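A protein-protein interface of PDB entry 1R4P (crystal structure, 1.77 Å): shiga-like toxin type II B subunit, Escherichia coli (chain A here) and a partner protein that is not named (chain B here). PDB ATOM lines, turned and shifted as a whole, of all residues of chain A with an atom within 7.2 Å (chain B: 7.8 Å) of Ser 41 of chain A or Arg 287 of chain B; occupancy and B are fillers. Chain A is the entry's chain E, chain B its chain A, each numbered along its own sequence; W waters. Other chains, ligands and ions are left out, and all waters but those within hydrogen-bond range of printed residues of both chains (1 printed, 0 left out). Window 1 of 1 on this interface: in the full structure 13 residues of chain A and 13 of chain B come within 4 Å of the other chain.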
ATOM      1  N   ILE A   8      10.253  20.760 -20.742  1.00  0.00           N
ATOM      2  CA  ILE A   8       9.686  20.636 -19.404  1.00  0.00           C
ATOM      3  C   ILE A   8       9.212  19.219 -19.240  1.00  0.00           C
ATOM      4  O   ILE A   8       8.399  18.734 -20.042  1.00  0.00           O
ATOM      5  CB  ILE A   8       8.504  21.615 -19.242  1.00  0.00           C
ATOM      6  CG1 ILE A   8       9.049  23.064 -19.202  1.00  0.00           C
ATOM      7  CG2 ILE A   8       7.737  21.280 -17.975  1.00  0.00           C
ATOM      8  CD1 ILE A   8       7.923  24.109 -19.425  1.00  0.00           C
ATOM      9  N   LEU A  35       3.674  33.214 -15.736  1.00  0.00           N
ATOM     10  CA  LEU A  35       4.464  32.118 -16.288  1.00  0.00           C
ATOM     11  C   LEU A  35       3.742  30.796 -16.399  1.00  0.00           C
ATOM     12  O   LEU A  35       4.209  29.909 -17.086  1.00  0.00           O
ATOM     13  CB  LEU A  35       5.712  31.945 -15.426  1.00  0.00           C
ATOM     14  CG  LEU A  35       6.831  32.877 -15.852  1.00  0.00           C
ATOM     15  CD1 LEU A  35       7.919  32.667 -14.797  1.00  0.00           C
ATOM     16  CD2 LEU A  35       7.390  32.525 -17.248  1.00  0.00           C
ATOM     17  N   GLN A  36       2.590  30.652 -15.741  1.00  0.00           N
ATOM     18  CA  GLN A  36       1.923  29.352 -15.851  1.00  0.00           C
ATOM     19  C   GLN A  36       1.505  29.005 -17.254  1.00  0.00           C
ATOM     20  O   GLN A  36       1.837  27.941 -17.743  1.00  0.00           O
ATOM     21  CB  GLN A  36       0.743  29.258 -14.879  1.00  0.00           C
ATOM     22  CG  GLN A  36       1.297  29.224 -13.427  1.00  0.00           C
ATOM     23  CD  GLN A  36       0.223  28.982 -12.415  1.00  0.00           C
ATOM     24  OE1 GLN A  36      -0.800  28.390 -12.726  1.00  0.00           O
ATOM     25  NE2 GLN A  36       0.462  29.410 -11.177  1.00  0.00           N
ATOM     26  N   PRO A  37       0.741  29.874 -17.924  1.00  0.00           N
ATOM     27  CA  PRO A  37       0.366  29.489 -19.294  1.00  0.00           C
ATOM     28  C   PRO A  37       1.604  29.409 -20.189  1.00  0.00           C
ATOM     29  O   PRO A  37       1.656  28.609 -21.115  1.00  0.00           O
ATOM     30  CB  PRO A  37      -0.584  30.634 -19.756  1.00  0.00           C
ATOM     31  CG  PRO A  37      -0.272  31.792 -18.793  1.00  0.00           C
ATOM     32  CD  PRO A  37       0.029  31.083 -17.471  1.00  0.00           C
ATOM     33  N   LEU A  38       2.538  30.312 -19.979  1.00  0.00           N
ATOM     34  CA  LEU A  38       3.747  30.301 -20.821  1.00  0.00           C
ATOM     35  C   LEU A  38       4.507  28.997 -20.644  1.00  0.00           C
ATOM     36  O   LEU A  38       4.893  28.344 -21.632  1.00  0.00           O
ATOM     37  CB  LEU A  38       4.661  31.479 -20.481  1.00  0.00           C
ATOM     38  CG  LEU A  38       3.945  32.844 -20.688  1.00  0.00           C
ATOM     39  CD1 LEU A  38       4.903  33.944 -20.184  1.00  0.00           C
ATOM     40  CD2 LEU A  38       3.596  33.073 -22.142  1.00  0.00           C
ATOM     41  N   LEU A  39       4.696  28.590 -19.390  1.00  0.00           N
ATOM     42  CA  LEU A  39       5.423  27.369 -19.161  1.00  0.00           C
ATOM     43  C   LEU A  39       4.639  26.158 -19.605  1.00  0.00           C
ATOM     44  O   LEU A  39       5.192  25.212 -20.167  1.00  0.00           O
ATOM     45  CB  LEU A  39       5.769  27.215 -17.675  1.00  0.00           C
ATOM     46  CG  LEU A  39       6.812  28.233 -17.202  1.00  0.00           C
ATOM     47  CD1 LEU A  39       6.854  28.215 -15.662  1.00  0.00           C
ATOM     48  CD2 LEU A  39       8.202  27.887 -17.770  1.00  0.00           C
ATOM     49  N   GLN A  40       3.341  26.129 -19.303  1.00  0.00           N
ATOM     50  CA  GLN A  40       2.581  24.959 -19.733  1.00  0.00           C
ATOM     51  C   GLN A  40       2.530  24.895 -21.245  1.00  0.00           C
ATOM     52  O   GLN A  40       2.628  23.823 -21.830  1.00  0.00           O
ATOM     53  CB  GLN A  40       1.155  24.976 -19.179  1.00  0.00           C
ATOM     54  CG  GLN A  40       0.536  23.582 -19.430  1.00  0.00           C
ATOM     55  CD  GLN A  40      -0.937  23.616 -19.452  1.00  0.00           C
ATOM     56  OE1 GLN A  40      -1.519  24.492 -20.071  1.00  0.00           O
ATOM     57  NE2 GLN A  40      -1.565  22.659 -18.781  1.00  0.00           N
ATOM     58  N   SER A  41       2.383  26.038 -21.899  1.00  0.00           N
ATOM     59  CA  SER A  41       2.392  25.996 -23.358  1.00  0.00           C
ATOM     60  C   SER A  41       3.756  25.484 -23.842  1.00  0.00           C
ATOM     61  O   SER A  41       3.827  24.739 -24.813  1.00  0.00           O
ATOM     62  CB  SER A  41       2.138  27.386 -23.906  1.00  0.00           C
ATOM     63  OG  SER A  41       0.752  27.688 -23.773  1.00  0.00           O
ATOM     64  N   ALA A  42       4.838  25.930 -23.195  1.00  0.00           N
ATOM     65  CA  ALA A  42       6.168  25.449 -23.572  1.00  0.00           C
ATOM     66  C   ALA A  42       6.219  23.948 -23.363  1.00  0.00           C
ATOM     67  O   ALA A  42       6.775  23.215 -24.181  1.00  0.00           O
ATOM     68  CB  ALA A  42       7.237  26.152 -22.679  1.00  0.00           C
ATOM     69  N   GLN A  43       5.659  23.476 -22.243  1.00  0.00           N
ATOM     70  CA  GLN A  43       5.659  22.077 -21.981  1.00  0.00           C
ATOM     71  C   GLN A  43       4.908  21.273 -23.035  1.00  0.00           C
ATOM     72  O   GLN A  43       5.417  20.278 -23.546  1.00  0.00           O
ATOM     73  CB  GLN A  43       5.020  21.785 -20.601  1.00  0.00           C
ATOM     74  CG  GLN A  43       4.865  20.312 -20.326  1.00  0.00           C
ATOM     75  CD  GLN A  43       4.180  20.088 -18.959  1.00  0.00           C
ATOM     76  OE1 GLN A  43       3.806  21.062 -18.267  1.00  0.00           O
ATOM     77  NE2 GLN A  43       3.997  18.826 -18.585  1.00  0.00           N
ATOM     78  N   LEU A  44       3.696  21.699 -23.380  1.00  0.00           N
ATOM     79  CA  LEU A  44       2.907  20.896 -24.273  1.00  0.00           C
ATOM     80  C   LEU A  44       3.325  20.985 -25.741  1.00  0.00           C
ATOM     81  O   LEU A  44       2.939  20.154 -26.541  1.00  0.00           O
ATOM     82  CB  LEU A  44       1.443  21.237 -24.076  1.00  0.00           C
ATOM     83  CG  LEU A  44       1.011  22.620 -24.562  1.00  0.00           C
ATOM     84  CD1 LEU A  44       0.543  22.493 -26.027  1.00  0.00           C
ATOM     85  CD2 LEU A  44      -0.227  23.088 -23.686  1.00  0.00           C
ATOM     86  N   THR A  45       4.134  21.974 -26.061  1.00  0.00           N
ATOM     87  CA  THR A  45       4.613  22.170 -27.439  1.00  0.00           C
ATOM     88  C   THR A  45       6.085  21.781 -27.535  1.00  0.00           C
ATOM     89  O   THR A  45       6.678  21.903 -28.609  1.00  0.00           O
ATOM     90  CB  THR A  45       4.540  23.644 -27.900  1.00  0.00           C
ATOM     91  OG1 THR A  45       5.319  24.456 -26.994  1.00  0.00           O
ATOM     92  CG2 THR A  45       3.042  24.148 -27.942  1.00  0.00           C
ATOM     93  N   GLY A  46       6.676  21.346 -26.423  1.00  0.00           N
ATOM     94  CA  GLY A  46       8.067  20.900 -26.477  1.00  0.00           C
ATOM     95  C   GLY A  46       9.098  21.988 -26.710  1.00  0.00           C
ATOM     96  O   GLY A  46      10.186  21.762 -27.295  1.00  0.00           O
ATOM     97  N   MET A  47       8.789  23.188 -26.253  1.00  0.00           N
ATOM     98  CA  MET A  47       9.804  24.222 -26.360  1.00  0.00           C
ATOM     99  C   MET A  47      10.950  23.914 -25.425  1.00  0.00           C
ATOM    100  O   MET A  47      10.817  23.229 -24.431  1.00  0.00           O
ATOM    101  CB  MET A  47       9.256  25.580 -25.937  1.00  0.00           C
ATOM    102  CG  MET A  47       8.158  26.064 -26.845  1.00  0.00           C
ATOM    103  SD  MET A  47       7.698  27.745 -26.345  1.00  0.00           S
ATOM    104  CE  MET A  47       8.576  28.749 -27.537  1.00  0.00           C
ATOM    105  N   PHE A  67      12.490  30.954 -23.760  1.00  0.00           N
ATOM    106  CA  PHE A  67      11.728  29.948 -24.492  1.00  0.00           C
ATOM    107  C   PHE A  67      12.267  29.896 -25.898  1.00  0.00           C
ATOM    108  O   PHE A  67      12.366  30.936 -26.552  1.00  0.00           O
ATOM    109  CB  PHE A  67      10.243  30.359 -24.604  1.00  0.00           C
ATOM    110  CG  PHE A  67       9.545  30.490 -23.276  1.00  0.00           C
ATOM    111  CD1 PHE A  67       9.586  31.691 -22.561  1.00  0.00           C
ATOM    112  CD2 PHE A  67       8.893  29.396 -22.711  1.00  0.00           C
ATOM    113  CE1 PHE A  67       8.989  31.797 -21.295  1.00  0.00           C
ATOM    114  CE2 PHE A  67       8.300  29.495 -21.460  1.00  0.00           C
ATOM    115  CZ  PHE A  67       8.351  30.713 -20.744  1.00  0.00           C
ATOM    116  N   ARG B 219       3.652  19.485 -36.444  1.00  0.00           N
ATOM    117  CA  ARG B 219       3.836  19.707 -35.020  1.00  0.00           C
ATOM    118  C   ARG B 219       2.754  18.949 -34.327  1.00  0.00           C
ATOM    119  O   ARG B 219       1.591  19.147 -34.619  1.00  0.00           O
ATOM    120  CB  ARG B 219       3.737  21.212 -34.688  1.00  0.00           C
ATOM    121  CG  ARG B 219       4.889  22.012 -35.285  1.00  0.00           C
ATOM    122  CD  ARG B 219       6.226  21.834 -34.538  1.00  0.00           C
ATOM    123  NE  ARG B 219       6.184  22.546 -33.249  1.00  0.00           N
ATOM    124  CZ  ARG B 219       5.944  22.015 -32.055  1.00  0.00           C
ATOM    125  NH1 ARG B 219       5.734  20.684 -31.840  1.00  0.00           N
ATOM    126  NH2 ARG B 219       5.789  22.873 -31.056  1.00  0.00           N
ATOM    127  N   GLY B 221       1.973  18.172 -30.479  1.00  0.00           N
ATOM    128  CA  GLY B 221       2.437  18.298 -29.089  1.00  0.00           C
ATOM    129  C   GLY B 221       3.900  18.726 -29.042  1.00  0.00           C
ATOM    130  O   GLY B 221       4.329  19.733 -29.647  1.00  0.00           O
ATOM    131  N   ARG B 222       4.675  17.951 -28.312  1.00  0.00           N
ATOM    132  CA  ARG B 222       6.092  18.231 -28.137  1.00  0.00           C
ATOM    133  C   ARG B 222       6.940  17.762 -29.301  1.00  0.00           C
ATOM    134  O   ARG B 222       8.142  18.023 -29.319  1.00  0.00           O
ATOM    135  CB  ARG B 222       6.588  17.513 -26.870  1.00  0.00           C
ATOM    136  CG  ARG B 222       5.799  17.949 -25.594  1.00  0.00           C
ATOM    137  CD  ARG B 222       5.984  16.929 -24.493  1.00  0.00           C
ATOM    138  NE  ARG B 222       7.373  16.684 -24.078  1.00  0.00           N
ATOM    139  CZ  ARG B 222       8.065  17.444 -23.236  1.00  0.00           C
ATOM    140  NH1 ARG B 222       7.551  18.585 -22.710  1.00  0.00           N
ATOM    141  NH2 ARG B 222       9.215  16.966 -22.752  1.00  0.00           N
ATOM    142  N   THR B 280      -3.116  20.629 -30.224  1.00  0.00           N
ATOM    143  CA  THR B 280      -1.958  21.321 -29.702  1.00  0.00           C
ATOM    144  C   THR B 280      -2.154  22.817 -29.820  1.00  0.00           C
ATOM    145  O   THR B 280      -1.896  23.542 -28.874  1.00  0.00           O
ATOM    146  CB  THR B 280      -0.688  20.913 -30.485  1.00  0.00           C
ATOM    147  OG1 THR B 280      -0.440  19.530 -30.219  1.00  0.00           O
ATOM    148  CG2 THR B 280       0.495  21.710 -30.003  1.00  0.00           C
ATOM    149  N   ALA B 281      -2.554  23.292 -30.994  1.00  0.00           N
ATOM    150  CA  ALA B 281      -2.747  24.726 -31.144  1.00  0.00           C
ATOM    151  C   ALA B 281      -3.838  25.166 -30.173  1.00  0.00           C
ATOM    152  O   ALA B 281      -3.693  26.199 -29.524  1.00  0.00           O
ATOM    153  CB  ALA B 281      -3.174  25.079 -32.618  1.00  0.00           C
ATOM    154  N   ALA B 282      -4.928  24.393 -30.096  1.00  0.00           N
ATOM    155  CA  ALA B 282      -6.027  24.768 -29.185  1.00  0.00           C
ATOM    156  C   ALA B 282      -5.521  24.927 -27.777  1.00  0.00           C
ATOM    157  O   ALA B 282      -5.994  25.796 -27.063  1.00  0.00           O
ATOM    158  CB  ALA B 282      -7.129  23.718 -29.184  1.00  0.00           C
ATOM    159  N   ALA B 283      -4.553  24.101 -27.390  1.00  0.00           N
ATOM    160  CA  ALA B 283      -4.029  24.130 -26.018  1.00  0.00           C
ATOM    161  C   ALA B 283      -3.149  25.295 -25.666  1.00  0.00           C
ATOM    162  O   ALA B 283      -2.892  25.497 -24.491  1.00  0.00           O
ATOM    163  CB  ALA B 283      -3.354  22.797 -25.658  1.00  0.00           C
ATOM    164  N   PHE B 284      -2.635  26.033 -26.663  1.00  0.00           N
ATOM    165  CA  PHE B 284      -1.922  27.265 -26.295  1.00  0.00           C
ATOM    166  C   PHE B 284      -2.699  28.484 -26.798  1.00  0.00           C
ATOM    167  O   PHE B 284      -2.307  29.598 -26.561  1.00  0.00           O
ATOM    168  CB  PHE B 284      -0.462  27.288 -26.758  1.00  0.00           C
ATOM    169  CG  PHE B 284      -0.260  27.203 -28.242  1.00  0.00           C
ATOM    170  CD1 PHE B 284      -0.348  28.331 -29.024  1.00  0.00           C
ATOM    171  CD2 PHE B 284       0.119  26.007 -28.831  1.00  0.00           C
ATOM    172  CE1 PHE B 284      -0.038  28.291 -30.378  1.00  0.00           C
ATOM    173  CE2 PHE B 284       0.427  25.953 -30.194  1.00  0.00           C
ATOM    174  CZ  PHE B 284       0.358  27.095 -30.961  1.00  0.00           C
ATOM    175  N   LEU B 285      -3.854  28.282 -27.427  1.00  0.00           N
ATOM    176  CA  LEU B 285      -4.645  29.414 -27.887  1.00  0.00           C
ATOM    177  C   LEU B 285      -5.895  29.533 -27.010  1.00  0.00           C
ATOM    178  O   LEU B 285      -6.876  30.170 -27.380  1.00  0.00           O
ATOM    179  CB  LEU B 285      -5.081  29.190 -29.329  1.00  0.00           C
ATOM    180  CG  LEU B 285      -3.914  29.119 -30.333  1.00  0.00           C
ATOM    181  CD1 LEU B 285      -4.447  28.805 -31.694  1.00  0.00           C
ATOM    182  CD2 LEU B 285      -3.152  30.479 -30.334  1.00  0.00           C
ATOM    183  N   ASN B 286      -5.903  28.868 -25.872  1.00  0.00           N
ATOM    184  CA  ASN B 286      -7.091  28.931 -25.025  1.00  0.00           C
ATOM    185  C   ASN B 286      -6.815  29.788 -23.797  1.00  0.00           C
ATOM    186  O   ASN B 286      -7.463  29.600 -22.785  1.00  0.00           O
ATOM    187  CB  ASN B 286      -7.490  27.515 -24.596  1.00  0.00           C
ATOM    188  CG  ASN B 286      -6.446  26.875 -23.690  1.00  0.00           C
ATOM    189  OD1 ASN B 286      -5.318  27.371 -23.586  1.00  0.00           O
ATOM    190  ND2 ASN B 286      -6.811  25.760 -23.031  1.00  0.00           N
ATOM    191  N   ARG B 287      -5.860  30.710 -23.907  1.00  0.00           N
ATOM    192  CA  ARG B 287      -5.548  31.593 -22.798  1.00  0.00           C
ATOM    193  C   ARG B 287      -6.317  32.900 -22.940  1.00  0.00           C
ATOM    194  O   ARG B 287      -6.450  33.398 -24.048  1.00  0.00           O
ATOM    195  CB  ARG B 287      -4.068  31.948 -22.785  1.00  0.00           C
ATOM    196  CG  ARG B 287      -3.180  30.838 -22.252  1.00  0.00           C
ATOM    197  CD  ARG B 287      -3.007  29.615 -23.182  1.00  0.00           C
ATOM    198  NE  ARG B 287      -1.932  28.769 -22.636  1.00  0.00           N
ATOM    199  CZ  ARG B 287      -2.118  27.634 -21.975  1.00  0.00           C
ATOM    200  NH1 ARG B 287      -3.329  27.130 -21.719  1.00  0.00           N
ATOM    201  NH2 ARG B 287      -1.043  26.956 -21.565  1.00  0.00           N
ATOM    202  N   LYS B 288      -6.796  33.457 -21.826  1.00  0.00           N
ATOM    203  CA  LYS B 288      -7.451  34.762 -21.965  1.00  0.00           C
ATOM    204  C   LYS B 288      -6.348  35.828 -21.818  1.00  0.00           C
ATOM    205  O   LYS B 288      -5.152  35.530 -21.780  1.00  0.00           O
ATOM    206  CB  LYS B 288      -8.518  34.985 -20.890  1.00  0.00           C
ATOM    207  CG  LYS B 288      -7.979  35.060 -19.514  1.00  0.00           C
ATOM    208  CD  LYS B 288      -9.187  35.302 -18.536  1.00  0.00           C
ATOM    209  CE  LYS B 288      -8.701  35.276 -17.126  1.00  0.00           C
ATOM    210  NZ  LYS B 288      -9.818  35.602 -16.170  1.00  0.00           N
ATOM    211  N   SER B 289      -6.763  37.081 -21.776  1.00  0.00           N
ATOM    212  CA  SER B 289      -5.827  38.191 -21.663  1.00  0.00           C
ATOM    213  C   SER B 289      -4.948  37.915 -20.445  1.00  0.00           C
ATOM    214  O   SER B 289      -5.433  37.656 -19.337  1.00  0.00           O
ATOM    215  CB  SER B 289      -6.640  39.483 -21.499  1.00  0.00           C
ATOM    216  OG  SER B 289      -5.805  40.539 -21.037  1.00  0.00           O
ATOM    217  N   GLN B 290      -3.654  38.051 -20.657  1.00  0.00           N
ATOM    218  CA  GLN B 290      -2.655  37.726 -19.640  1.00  0.00           C
ATOM    219  C   GLN B 290      -2.851  38.614 -18.426  1.00  0.00           C
ATOM    220  O   GLN B 290      -2.786  38.156 -17.294  1.00  0.00           O
ATOM    221  CB  GLN B 290      -1.248  37.966 -20.192  1.00  0.00           C
ATOM    222  CG  GLN B 290      -0.111  37.542 -19.284  1.00  0.00           C
ATOM    223  CD  GLN B 290       0.120  36.053 -19.271  1.00  0.00           C
ATOM    224  OE1 GLN B 290      -0.839  35.251 -19.313  1.00  0.00           O
ATOM    225  NE2 GLN B 290       1.391  35.654 -19.175  1.00  0.00           N
ATOM    226  N   TYR B 293      -5.670  37.351 -16.547  1.00  0.00           N
ATOM    227  CA  TYR B 293      -5.393  36.048 -15.995  1.00  0.00           C
ATOM    228  C   TYR B 293      -4.611  36.146 -14.701  1.00  0.00           C
ATOM    229  O   TYR B 293      -4.992  35.577 -13.661  1.00  0.00           O
ATOM    230  CB  TYR B 293      -4.571  35.245 -16.991  1.00  0.00           C
ATOM    231  CG  TYR B 293      -4.152  33.903 -16.476  1.00  0.00           C
ATOM    232  CD1 TYR B 293      -5.048  32.832 -16.450  1.00  0.00           C
ATOM    233  CD2 TYR B 293      -2.837  33.706 -16.046  1.00  0.00           C
ATOM    234  CE1 TYR B 293      -4.628  31.575 -16.008  1.00  0.00           C
ATOM    235  CE2 TYR B 293      -2.393  32.449 -15.602  1.00  0.00           C
ATOM    236  CZ  TYR B 293      -3.276  31.409 -15.595  1.00  0.00           C
ATOM    237  OH  TYR B 293      -2.813  30.153 -15.242  1.00  0.00           O
HETATM  238  O   HOH W   1       0.512  30.361 -23.677  1.00  0.00           O
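Water W1 lies within hydrogen-bond range of the side-chain hydroxyl of Ser 41 of chain A (2.7 Å), the guanidinium group of Arg 287 of chain B (3.1 Å) and the backbone carbonyl oxygen of Pro 37 of chain A (3.3 Å).
Leu 35 of chain A touches none of the printed residues of chain B. Of the printed residues of chain B, Gln 36 of chain A touches Tyr 293 (3.7 Å). Of the printed residues of chain B, Gln 40 of chain A touches Arg 287. Of chain B, only Phe 284 (3.2 Å) and Arg 287 (2.9 Å) come within 4 Å of Ser 41 of chain A. No residue of chain B comes within 4 Å of Ala 42 of chain A. Of chain A, only Pro 37 (3.2 Å), Gln 40 (2.9 Å) and Ser 41 (2.9 Å) come within 4 Å of Arg 287 of chain B. Ser 289 of chain B touches none of the printed residues of chain A. The nearest residue of chain B that does not touch Ser 41 of chain A is Ala 283 of chain B (4.3 Å). The nearest printed residue of chain B that does not touch Leu 44 of chain A is Arg 287 of chain B (4.5 Å).
Of the 15 printed residues of chain B, 9 touch a printed residue of chain A. Hydrophobic or aromatic side chains of chain B that line the printed part of chain A: Ala 283, Phe 284 and Tyr 293. Of the 15 printed residues of chain A, 9 touch a printed residue of chain B.
NH2 of Arg 287 of chain B sits at hydrogen-bond distance from O of Pro 37 of chain A, at 3.2 Å. O of Leu 44 of chain A lies close to O of Gly 221 of chain B, at 3.4 Å. The backbone NH (N) of Arg 222 of chain B sits at hydrogen-bond distance from the backbone carbonyl oxygen (O) of Leu 44 of chain A (3.3 Å). OG of Ser 41 of chain A sits at hydrogen-bond distance from NH2 of Arg 287 of chain B (2.9 Å). NH1 of Arg 222 of chain B lies within hydrogen-bond range of O of Ile 8 of chain A (2.8 Å). The backbone carbonyl oxygen (O) of Gln 43 of chain A lies within hydrogen-bond range of the guanidinium group (NH1) of Arg 222 of chain B (2.8 Å). The guanidinium group (NH2) of Arg 219 of chain B sits at hydrogen-bond distance from the backbone carbonyl oxygen (O) of Thr 45 of chain A (2.8 Å). The backbone carbonyl oxygen (O) of Thr 45 of chain A lies close to the backbone carbonyl oxygen (O) of Gly 221 of chain B, at 3.4 Å. The guanidinium group of Arg 287 of chain B lies within hydrogen-bond range of the side-chain amide oxygen of Gln 40 of chain A, at 2.9 Å.
Among the printed residues, merely in contact across the chains: Ser 41 of chain A with Phe 284 of chain B, Pro 37 of chain A with Tyr 293 of chain B, Pro 37 of chain A with Gln 290 of chain B, Thr 45 of chain A with Phe 284 of chain B, Thr 45 of chain A with Arg 222 of chain B, Gly 46 of chain A with Arg 222 of chain B, Gln 36 of chain A with Tyr 293 of chain B, Leu 44 of chain A with Ala 283 of chain B and Leu 44 of chain A with Thr 280 of chain B.
O of Ala 283 of chain B is in hydrogen-bond range of NH1 of Arg 287 of chain B (3.2 Å). O of Pro 37 of chain A sits at hydrogen-bond distance from OG of Ser 41 of chain A, 3.0 Å away. The backbone NH (N) of Gly 221 of chain B sits at hydrogen-bond distance from the side-chain hydroxyl (OG1) of Thr 280 of chain B (2.8 Å). The backbone carbonyl oxygen (O) of Ala 283 of chain B sits close to the side-chain amide oxygen (OD1) of Asn 286 of chain B (3.2 Å). O of Ser 41 of chain A sits at hydrogen-bond distance from OG1 of Thr 45 of chain A. O of Ala 42 of chain A is in hydrogen-bond range of OG1 of Thr 45 of chain A, at 3.4 Å.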
